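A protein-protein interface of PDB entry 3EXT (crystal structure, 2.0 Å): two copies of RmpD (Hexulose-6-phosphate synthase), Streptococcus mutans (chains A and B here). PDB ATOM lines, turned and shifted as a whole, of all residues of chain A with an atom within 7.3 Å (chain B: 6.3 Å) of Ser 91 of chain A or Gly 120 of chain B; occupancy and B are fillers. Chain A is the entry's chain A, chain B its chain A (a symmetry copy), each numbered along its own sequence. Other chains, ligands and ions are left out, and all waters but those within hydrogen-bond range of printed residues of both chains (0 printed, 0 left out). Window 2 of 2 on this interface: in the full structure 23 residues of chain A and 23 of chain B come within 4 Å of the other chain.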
ATOM      1  N   CYS A  67      31.549 -17.555  22.314  1.00  0.00           N
ATOM      2  CA  CYS A  67      32.064 -17.255  23.658  1.00  0.00           C
ATOM      3  C   CYS A  67      31.182 -17.906  24.751  1.00  0.00           C
ATOM      4  O   CYS A  67      29.977 -17.723  24.739  1.00  0.00           O
ATOM      5  CB  CYS A  67      32.042 -15.752  23.790  1.00  0.00           C
ATOM      6  SG  CYS A  67      32.613 -15.116  25.338  1.00  0.00           S
ATOM      7  N   ALA A  68      31.791 -18.651  25.690  1.00  0.00           N
ATOM      8  CA  ALA A  68      31.091 -19.250  26.832  1.00  0.00           C
ATOM      9  C   ALA A  68      31.396 -18.559  28.179  1.00  0.00           C
ATOM     10  O   ALA A  68      30.672 -18.789  29.142  1.00  0.00           O
ATOM     11  CB  ALA A  68      31.427 -20.763  26.957  1.00  0.00           C
ATOM     12  N   CYS A  88      27.986 -15.643  21.097  1.00  0.00           N
ATOM     13  CA  CYS A  88      28.121 -16.326  22.375  1.00  0.00           C
ATOM     14  C   CYS A  88      27.324 -17.605  22.247  1.00  0.00           C
ATOM     15  O   CYS A  88      26.244 -17.580  21.664  1.00  0.00           O
ATOM     16  CB  CYS A  88      27.514 -15.486  23.535  1.00  0.00           C
ATOM     17  SG  CYS A  88      28.558 -14.123  24.156  1.00  0.00           S
ATOM     18  N   ILE A  89      27.850 -18.695  22.804  1.00  0.00           N
ATOM     19  CA  ILE A  89      27.173 -19.978  22.825  1.00  0.00           C
ATOM     20  C   ILE A  89      26.003 -19.860  23.836  1.00  0.00           C
ATOM     21  O   ILE A  89      26.117 -19.176  24.872  1.00  0.00           O
ATOM     22  CB  ILE A  89      28.151 -21.156  23.147  1.00  0.00           C
ATOM     23  CG1 ILE A  89      27.555 -22.520  22.871  1.00  0.00           C
ATOM     24  CG2 ILE A  89      28.591 -21.162  24.606  1.00  0.00           C
ATOM     25  CD1 ILE A  89      27.242 -22.782  21.434  1.00  0.00           C
ATOM     26  N   CYS A  90      24.900 -20.512  23.528  1.00  0.00           N
ATOM     27  CA  CYS A  90      23.690 -20.360  24.362  1.00  0.00           C
ATOM     28  C   CYS A  90      23.909 -20.804  25.793  1.00  0.00           C
ATOM     29  O   CYS A  90      23.132 -20.423  26.660  1.00  0.00           O
ATOM     30  CB  CYS A  90      22.485 -21.086  23.755  1.00  0.00           C
ATOM     31  SG  CYS A  90      22.771 -22.810  23.399  1.00  0.00           S
ATOM     32  N   SER A  91      24.910 -21.626  26.055  1.00  0.00           N
ATOM     33  CA  SER A  91      25.139 -22.018  27.452  1.00  0.00           C
ATOM     34  C   SER A  91      25.895 -20.986  28.296  1.00  0.00           C
ATOM     35  O   SER A  91      26.015 -21.134  29.541  1.00  0.00           O
ATOM     36  CB  SER A  91      25.704 -23.429  27.598  1.00  0.00           C
ATOM     37  OG  SER A  91      26.636 -23.729  26.614  1.00  0.00           O
ATOM     38  N   ALA A  92      26.375 -19.930  27.641  1.00  0.00           N
ATOM     39  CA  ALA A  92      26.980 -18.814  28.342  1.00  0.00           C
ATOM     40  C   ALA A  92      25.953 -18.265  29.324  1.00  0.00           C
ATOM     41  O   ALA A  92      24.764 -18.147  28.979  1.00  0.00           O
ATOM     42  CB  ALA A  92      27.399 -17.720  27.367  1.00  0.00           C
ATOM     43  N   THR A  93      26.417 -17.864  30.516  1.00  0.00           N
ATOM     44  CA  THR A  93      25.507 -17.230  31.490  1.00  0.00           C
ATOM     45  C   THR A  93      25.069 -15.821  31.055  1.00  0.00           C
ATOM     46  O   THR A  93      25.636 -15.215  30.135  1.00  0.00           O
ATOM     47  CB  THR A  93      26.079 -17.208  32.882  1.00  0.00           C
ATOM     48  OG1 THR A  93      27.195 -16.308  32.922  1.00  0.00           O
ATOM     49  CG2 THR A  93      26.541 -18.643  33.288  1.00  0.00           C
ATOM     50  N   ILE A  94      24.008 -15.321  31.678  1.00  0.00           N
ATOM     51  CA  ILE A  94      23.563 -13.960  31.425  1.00  0.00           C
ATOM     52  C   ILE A  94      24.621 -12.900  31.810  1.00  0.00           C
ATOM     53  O   ILE A  94      24.816 -11.941  31.042  1.00  0.00           O
ATOM     54  CB  ILE A  94      22.162 -13.652  32.063  1.00  0.00           C
ATOM     55  CG1 ILE A  94      21.083 -14.612  31.535  1.00  0.00           C
ATOM     56  CG2 ILE A  94      21.735 -12.251  31.768  1.00  0.00           C
ATOM     57  CD1 ILE A  94      20.726 -14.442  30.093  1.00  0.00           C
ATOM     58  N   THR A  96      27.833 -13.340  31.710  1.00  0.00           N
ATOM     59  CA  THR A  96      28.810 -13.424  30.598  1.00  0.00           C
ATOM     60  C   THR A  96      28.309 -12.680  29.331  1.00  0.00           C
ATOM     61  O   THR A  96      29.049 -11.884  28.733  1.00  0.00           O
ATOM     62  CB  THR A  96      29.175 -14.871  30.250  1.00  0.00           C
ATOM     63  OG1 THR A  96      29.889 -15.481  31.378  1.00  0.00           O
ATOM     64  CG2 THR A  96      30.003 -14.923  28.934  1.00  0.00           C
ATOM     65  N   MET A  97      27.074 -12.933  28.916  1.00  0.00           N
ATOM     66  CA  MET A  97      26.588 -12.303  27.662  1.00  0.00           C
ATOM     67  C   MET A  97      26.472 -10.797  27.776  1.00  0.00           C
ATOM     68  O   MET A  97      26.748 -10.073  26.813  1.00  0.00           O
ATOM     69  CB  MET A  97      25.248 -12.887  27.245  1.00  0.00           C
ATOM     70  CG  MET A  97      25.299 -14.315  26.796  1.00  0.00           C
ATOM     71  SD  MET A  97      23.644 -14.813  26.315  1.00  0.00           S
ATOM     72  CE  MET A  97      23.907 -16.451  25.609  1.00  0.00           C
ATOM     73  N   VAL A 116      23.323 -14.957  19.732  1.00  0.00           N
ATOM     74  CA  VAL A 116      23.324 -16.225  20.477  1.00  0.00           C
ATOM     75  C   VAL A 116      23.335 -17.398  19.524  1.00  0.00           C
ATOM     76  O   VAL A 116      22.415 -17.554  18.691  1.00  0.00           O
ATOM     77  CB  VAL A 116      22.107 -16.362  21.471  1.00  0.00           C
ATOM     78  CG1 VAL A 116      22.262 -17.621  22.325  1.00  0.00           C
ATOM     79  CG2 VAL A 116      22.046 -15.139  22.400  1.00  0.00           C
ATOM     80  N   GLU A 117      24.376 -18.218  19.631  1.00  0.00           N
ATOM     81  CA  GLU A 117      24.483 -19.466  18.868  1.00  0.00           C
ATOM     82  C   GLU A 117      23.680 -20.555  19.561  1.00  0.00           C
ATOM     83  O   GLU A 117      23.991 -20.938  20.694  1.00  0.00           O
ATOM     84  CB  GLU A 117      25.947 -19.900  18.676  1.00  0.00           C
ATOM     85  CG  GLU A 117      26.680 -19.257  17.480  1.00  0.00           C
ATOM     86  CD  GLU A 117      26.316 -19.962  16.140  1.00  0.00           C
ATOM     87  OE1 GLU A 117      25.377 -20.779  16.151  1.00  0.00           O
ATOM     88  OE2 GLU A 117      26.906 -19.678  15.082  1.00  0.00           O
ATOM     89  N   TYR A 119      22.574 -24.144  20.258  1.00  0.00           N
ATOM     90  CA  TYR A 119      23.047 -25.555  20.277  1.00  0.00           C
ATOM     91  C   TYR A 119      22.410 -26.301  21.451  1.00  0.00           C
ATOM     92  O   TYR A 119      22.263 -25.732  22.544  1.00  0.00           O
ATOM     93  CB  TYR A 119      24.609 -25.690  20.398  1.00  0.00           C
ATOM     94  CG  TYR A 119      25.336 -25.425  19.081  1.00  0.00           C
ATOM     95  CD1 TYR A 119      25.758 -26.473  18.266  1.00  0.00           C
ATOM     96  CD2 TYR A 119      25.537 -24.115  18.625  1.00  0.00           C
ATOM     97  CE1 TYR A 119      26.341 -26.205  17.006  1.00  0.00           C
ATOM     98  CE2 TYR A 119      26.159 -23.840  17.390  1.00  0.00           C
ATOM     99  CZ  TYR A 119      26.551 -24.891  16.598  1.00  0.00           C
ATOM    100  OH  TYR A 119      27.165 -24.639  15.403  1.00  0.00           O
ATOM    101  N   TRP A 122      18.301 -25.667  24.532  1.00  0.00           N
ATOM    102  CA  TRP A 122      17.961 -24.317  24.991  1.00  0.00           C
ATOM    103  C   TRP A 122      16.443 -24.188  25.133  1.00  0.00           C
ATOM    104  O   TRP A 122      15.684 -24.945  24.501  1.00  0.00           O
ATOM    105  CB  TRP A 122      18.492 -23.262  23.987  1.00  0.00           C
ATOM    106  CG  TRP A 122      17.956 -23.424  22.599  1.00  0.00           C
ATOM    107  CD1 TRP A 122      18.433 -24.248  21.625  1.00  0.00           C
ATOM    108  CD2 TRP A 122      16.819 -22.738  22.027  1.00  0.00           C
ATOM    109  NE1 TRP A 122      17.681 -24.103  20.464  1.00  0.00           N
ATOM    110  CE2 TRP A 122      16.678 -23.197  20.695  1.00  0.00           C
ATOM    111  CE3 TRP A 122      15.910 -21.785  22.518  1.00  0.00           C
ATOM    112  CZ2 TRP A 122      15.652 -22.734  19.838  1.00  0.00           C
ATOM    113  CZ3 TRP A 122      14.885 -21.339  21.680  1.00  0.00           C
ATOM    114  CH2 TRP A 122      14.780 -21.810  20.343  1.00  0.00           C
ATOM    115  N   GLN A 126      14.950 -19.123  28.509  1.00  0.00           N
ATOM    116  CA  GLN A 126      16.351 -18.680  28.310  1.00  0.00           C
ATOM    117  C   GLN A 126      16.355 -17.568  27.274  1.00  0.00           C
ATOM    118  O   GLN A 126      16.861 -16.484  27.532  1.00  0.00           O
ATOM    119  CB  GLN A 126      17.233 -19.820  27.840  1.00  0.00           C
ATOM    120  CG  GLN A 126      17.644 -20.776  28.952  1.00  0.00           C
ATOM    121  CD  GLN A 126      18.352 -22.017  28.434  1.00  0.00           C
ATOM    122  OE1 GLN A 126      18.779 -22.053  27.293  1.00  0.00           O
ATOM    123  NE2 GLN A 126      18.502 -23.038  29.290  1.00  0.00           N
ATOM    124  N   TRP A 130      17.689 -13.562  27.195  1.00  0.00           N
ATOM    125  CA  TRP A 130      18.679 -12.937  26.280  1.00  0.00           C
ATOM    126  C   TRP A 130      18.171 -11.586  25.808  1.00  0.00           C
ATOM    127  O   TRP A 130      18.928 -10.619  25.750  1.00  0.00           O
ATOM    128  CB  TRP A 130      19.026 -13.824  25.067  1.00  0.00           C
ATOM    129  CG  TRP A 130      19.512 -15.192  25.442  1.00  0.00           C
ATOM    130  CD1 TRP A 130      20.245 -15.526  26.529  1.00  0.00           C
ATOM    131  CD2 TRP A 130      19.314 -16.397  24.696  1.00  0.00           C
ATOM    132  NE1 TRP A 130      20.497 -16.884  26.537  1.00  0.00           N
ATOM    133  CE2 TRP A 130      19.927 -17.444  25.426  1.00  0.00           C
ATOM    134  CE3 TRP A 130      18.629 -16.704  23.496  1.00  0.00           C
ATOM    135  CZ2 TRP A 130      19.894 -18.787  24.994  1.00  0.00           C
ATOM    136  CZ3 TRP A 130      18.601 -18.027  23.059  1.00  0.00           C
ATOM    137  CH2 TRP A 130      19.214 -19.057  23.811  1.00  0.00           C
ATOM    138  N   ILE B  89      32.201 -27.827  24.720  1.00  0.00           N
ATOM    139  CA  ILE B  89      31.201 -27.166  25.538  1.00  0.00           C
ATOM    140  C   ILE B  89      30.020 -28.157  25.704  1.00  0.00           C
ATOM    141  O   ILE B  89      29.689 -28.922  24.777  1.00  0.00           O
ATOM    142  CB  ILE B  89      30.770 -25.785  24.943  1.00  0.00           C
ATOM    143  CG1 ILE B  89      29.977 -24.937  25.914  1.00  0.00           C
ATOM    144  CG2 ILE B  89      29.907 -25.936  23.695  1.00  0.00           C
ATOM    145  CD1 ILE B  89      30.735 -24.510  27.128  1.00  0.00           C
ATOM    146  N   CYS B  90      29.407 -28.142  26.871  1.00  0.00           N
ATOM    147  CA  CYS B  90      28.355 -29.134  27.170  1.00  0.00           C
ATOM    148  C   CYS B  90      27.182 -29.045  26.217  1.00  0.00           C
ATOM    149  O   CYS B  90      26.418 -29.998  26.121  1.00  0.00           O
ATOM    150  CB  CYS B  90      27.873 -29.035  28.622  1.00  0.00           C
ATOM    151  SG  CYS B  90      27.334 -27.405  29.105  1.00  0.00           S
ATOM    152  N   SER B  91      26.994 -27.921  25.548  1.00  0.00           N
ATOM    153  CA  SER B  91      25.878 -27.859  24.595  1.00  0.00           C
ATOM    154  C   SER B  91      26.153 -28.507  23.234  1.00  0.00           C
ATOM    155  O   SER B  91      25.229 -28.658  22.392  1.00  0.00           O
ATOM    156  CB  SER B  91      25.266 -26.464  24.472  1.00  0.00           C
ATOM    157  OG  SER B  91      26.225 -25.462  24.509  1.00  0.00           O
ATOM    158  N   LEU B 118      31.511 -27.610  31.619  1.00  0.00           N
ATOM    159  CA  LEU B 118      30.160 -27.508  32.228  1.00  0.00           C
ATOM    160  C   LEU B 118      29.715 -26.065  32.441  1.00  0.00           C
ATOM    161  O   LEU B 118      30.193 -25.399  33.336  1.00  0.00           O
ATOM    162  CB  LEU B 118      30.127 -28.275  33.551  1.00  0.00           C
ATOM    163  CG  LEU B 118      30.424 -29.772  33.510  1.00  0.00           C
ATOM    164  CD1 LEU B 118      30.396 -30.382  34.891  1.00  0.00           C
ATOM    165  CD2 LEU B 118      29.445 -30.456  32.553  1.00  0.00           C
ATOM    166  N   TYR B 119      28.799 -25.600  31.611  1.00  0.00           N
ATOM    167  CA  TYR B 119      28.239 -24.222  31.635  1.00  0.00           C
ATOM    168  C   TYR B 119      26.713 -24.278  31.545  1.00  0.00           C
ATOM    169  O   TYR B 119      26.164 -25.106  30.800  1.00  0.00           O
ATOM    170  CB  TYR B 119      28.767 -23.310  30.468  1.00  0.00           C
ATOM    171  CG  TYR B 119      30.179 -22.781  30.714  1.00  0.00           C
ATOM    172  CD1 TYR B 119      30.391 -21.497  31.212  1.00  0.00           C
ATOM    173  CD2 TYR B 119      31.296 -23.601  30.510  1.00  0.00           C
ATOM    174  CE1 TYR B 119      31.700 -21.062  31.524  1.00  0.00           C
ATOM    175  CE2 TYR B 119      32.609 -23.158  30.777  1.00  0.00           C
ATOM    176  CZ  TYR B 119      32.790 -21.894  31.281  1.00  0.00           C
ATOM    177  OH  TYR B 119      34.057 -21.447  31.535  1.00  0.00           O
ATOM    178  N   GLY B 120      26.044 -23.367  32.231  1.00  0.00           N
ATOM    179  CA  GLY B 120      24.585 -23.256  32.121  1.00  0.00           C
ATOM    180  C   GLY B 120      23.852 -24.481  32.650  1.00  0.00           C
ATOM    181  O   GLY B 120      24.373 -25.202  33.522  1.00  0.00           O
ATOM    182  N   ASP B 121      22.654 -24.729  32.115  1.00  0.00           N
ATOM    183  CA  ASP B 121      21.764 -25.743  32.684  1.00  0.00           C
ATOM    184  C   ASP B 121      21.922 -27.126  32.066  1.00  0.00           C
ATOM    185  O   ASP B 121      21.028 -27.579  31.357  1.00  0.00           O
ATOM    186  CB  ASP B 121      20.281 -25.316  32.564  1.00  0.00           C
ATOM    187  CG  ASP B 121      19.946 -24.057  33.373  1.00  0.00           C
ATOM    188  OD1 ASP B 121      20.362 -23.951  34.554  1.00  0.00           O
ATOM    189  OD2 ASP B 121      19.240 -23.172  32.819  1.00  0.00           O
ATOM    190  N   TRP B 122      23.021 -27.809  32.369  1.00  0.00           N
ATOM    191  CA  TRP B 122      23.262 -29.196  31.959  1.00  0.00           C
ATOM    192  C   TRP B 122      22.560 -30.149  32.929  1.00  0.00           C
ATOM    193  O   TRP B 122      22.277 -29.780  34.083  1.00  0.00           O
ATOM    194  CB  TRP B 122      24.784 -29.490  31.936  1.00  0.00           C
ATOM    195  CG  TRP B 122      25.462 -29.274  33.253  1.00  0.00           C
ATOM    196  CD1 TRP B 122      25.934 -28.098  33.752  1.00  0.00           C
ATOM    197  CD2 TRP B 122      25.742 -30.279  34.254  1.00  0.00           C
ATOM    198  NE1 TRP B 122      26.518 -28.305  34.997  1.00  0.00           N
ATOM    199  CE2 TRP B 122      26.394 -29.630  35.330  1.00  0.00           C
ATOM    200  CE3 TRP B 122      25.497 -31.660  34.341  1.00  0.00           C
ATOM    201  CZ2 TRP B 122      26.809 -30.320  36.493  1.00  0.00           C
ATOM    202  CZ3 TRP B 122      25.888 -32.341  35.496  1.00  0.00           C
ATOM    203  CH2 TRP B 122      26.554 -31.663  36.552  1.00  0.00           C
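The side-chain hydroxyl of Ser 91 of chain B sits at hydrogen-bond distance from the side-chain hydroxyl of Ser 91 of chain A, at 2.8 Å.
O of Ser 91 of chain A sits at hydrogen-bond distance from N of Gly 120 of chain B (3.5 Å).
The backbone NH of Ile 89 of chain A sits at hydrogen-bond distance from the backbone carbonyl oxygen of Cys 67 of chain A (3.0 Å).
The side-chain sulfur (SG) of Cys 90 of chain A lies within hydrogen-bond range of the backbone carbonyl oxygen (O) of Tyr 119 of chain A (3.1 Å).
SG of Cys 90 of chain B lies within hydrogen-bond range of O of Tyr 119 of chain B, at 3.1 Å.
CD1 of Ile 89 of chain B touches CB of Ala 68 of chain A, at 3.8 Å.
Tyr 119 of chain B touches Ala 68 of chain A.
Ile 89 of chain A touches Ser 91 of chain B.
Ile 89 of chain B touches Ser 91 of chain A.
Ser 91 of chain A touches Tyr 119 of chain B (O to CB, 3.6 Å).
O of Ser 91 of chain B touches CB of Tyr 119 of chain A, 3.6 Å away.
NE2 of Gln 126 of chain A touches OD2 of Asp 121 of chain B, at 3.6 Å.
Of the printed residues of chain A, Asp 121 of chain B touches Gln 126.
Printed residues of chain A within 4 Å of Tyr 119 of chain B: Ala 68 (3.4 Å) and Ser 91 (3.6 Å).
Of the printed residues of chain A, Ser 91 of chain B touches Ile 89 (3.6 Å), Ser 91 (2.8 Å) and Tyr 119 (3.6 Å).
Of the printed residues of chain B, Ile 89 of chain A touches Ser 91 (3.6 Å).
Thr 93 of chain A touches none of the printed residues of chain B.
The nearest residue of chain B that does not touch Ser 91 of chain A is Cys 90 of chain B (4.5 Å).
Printed residues of chain A that touch a printed residue of chain B: Ala 68, Ile 89, Ser 91, Tyr 119 and Gln 126.
Hydrophobic or aromatic side chains of chain B within 4 Å of the printed part of chain A: Ile 89 and Tyr 119.
Along chain B the printed residues that touch a printed residue of chain A span positions 89 to 121.
Ile 89 of chain A touches Ser 91 of chain B, and with the chains exchanged Ser 91 of chain A touches Ile 89 of chain B.
Ser 91 of chain B touches its own counterpart, Ser 91 of chain A.
Ser 91 of chain A touches Tyr 119 of chain B, and with the chains exchanged Tyr 119 of chain A touches Ser 91 of chain B.
Positions printed for both chains: 89, 90, 91, 119 and 122.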
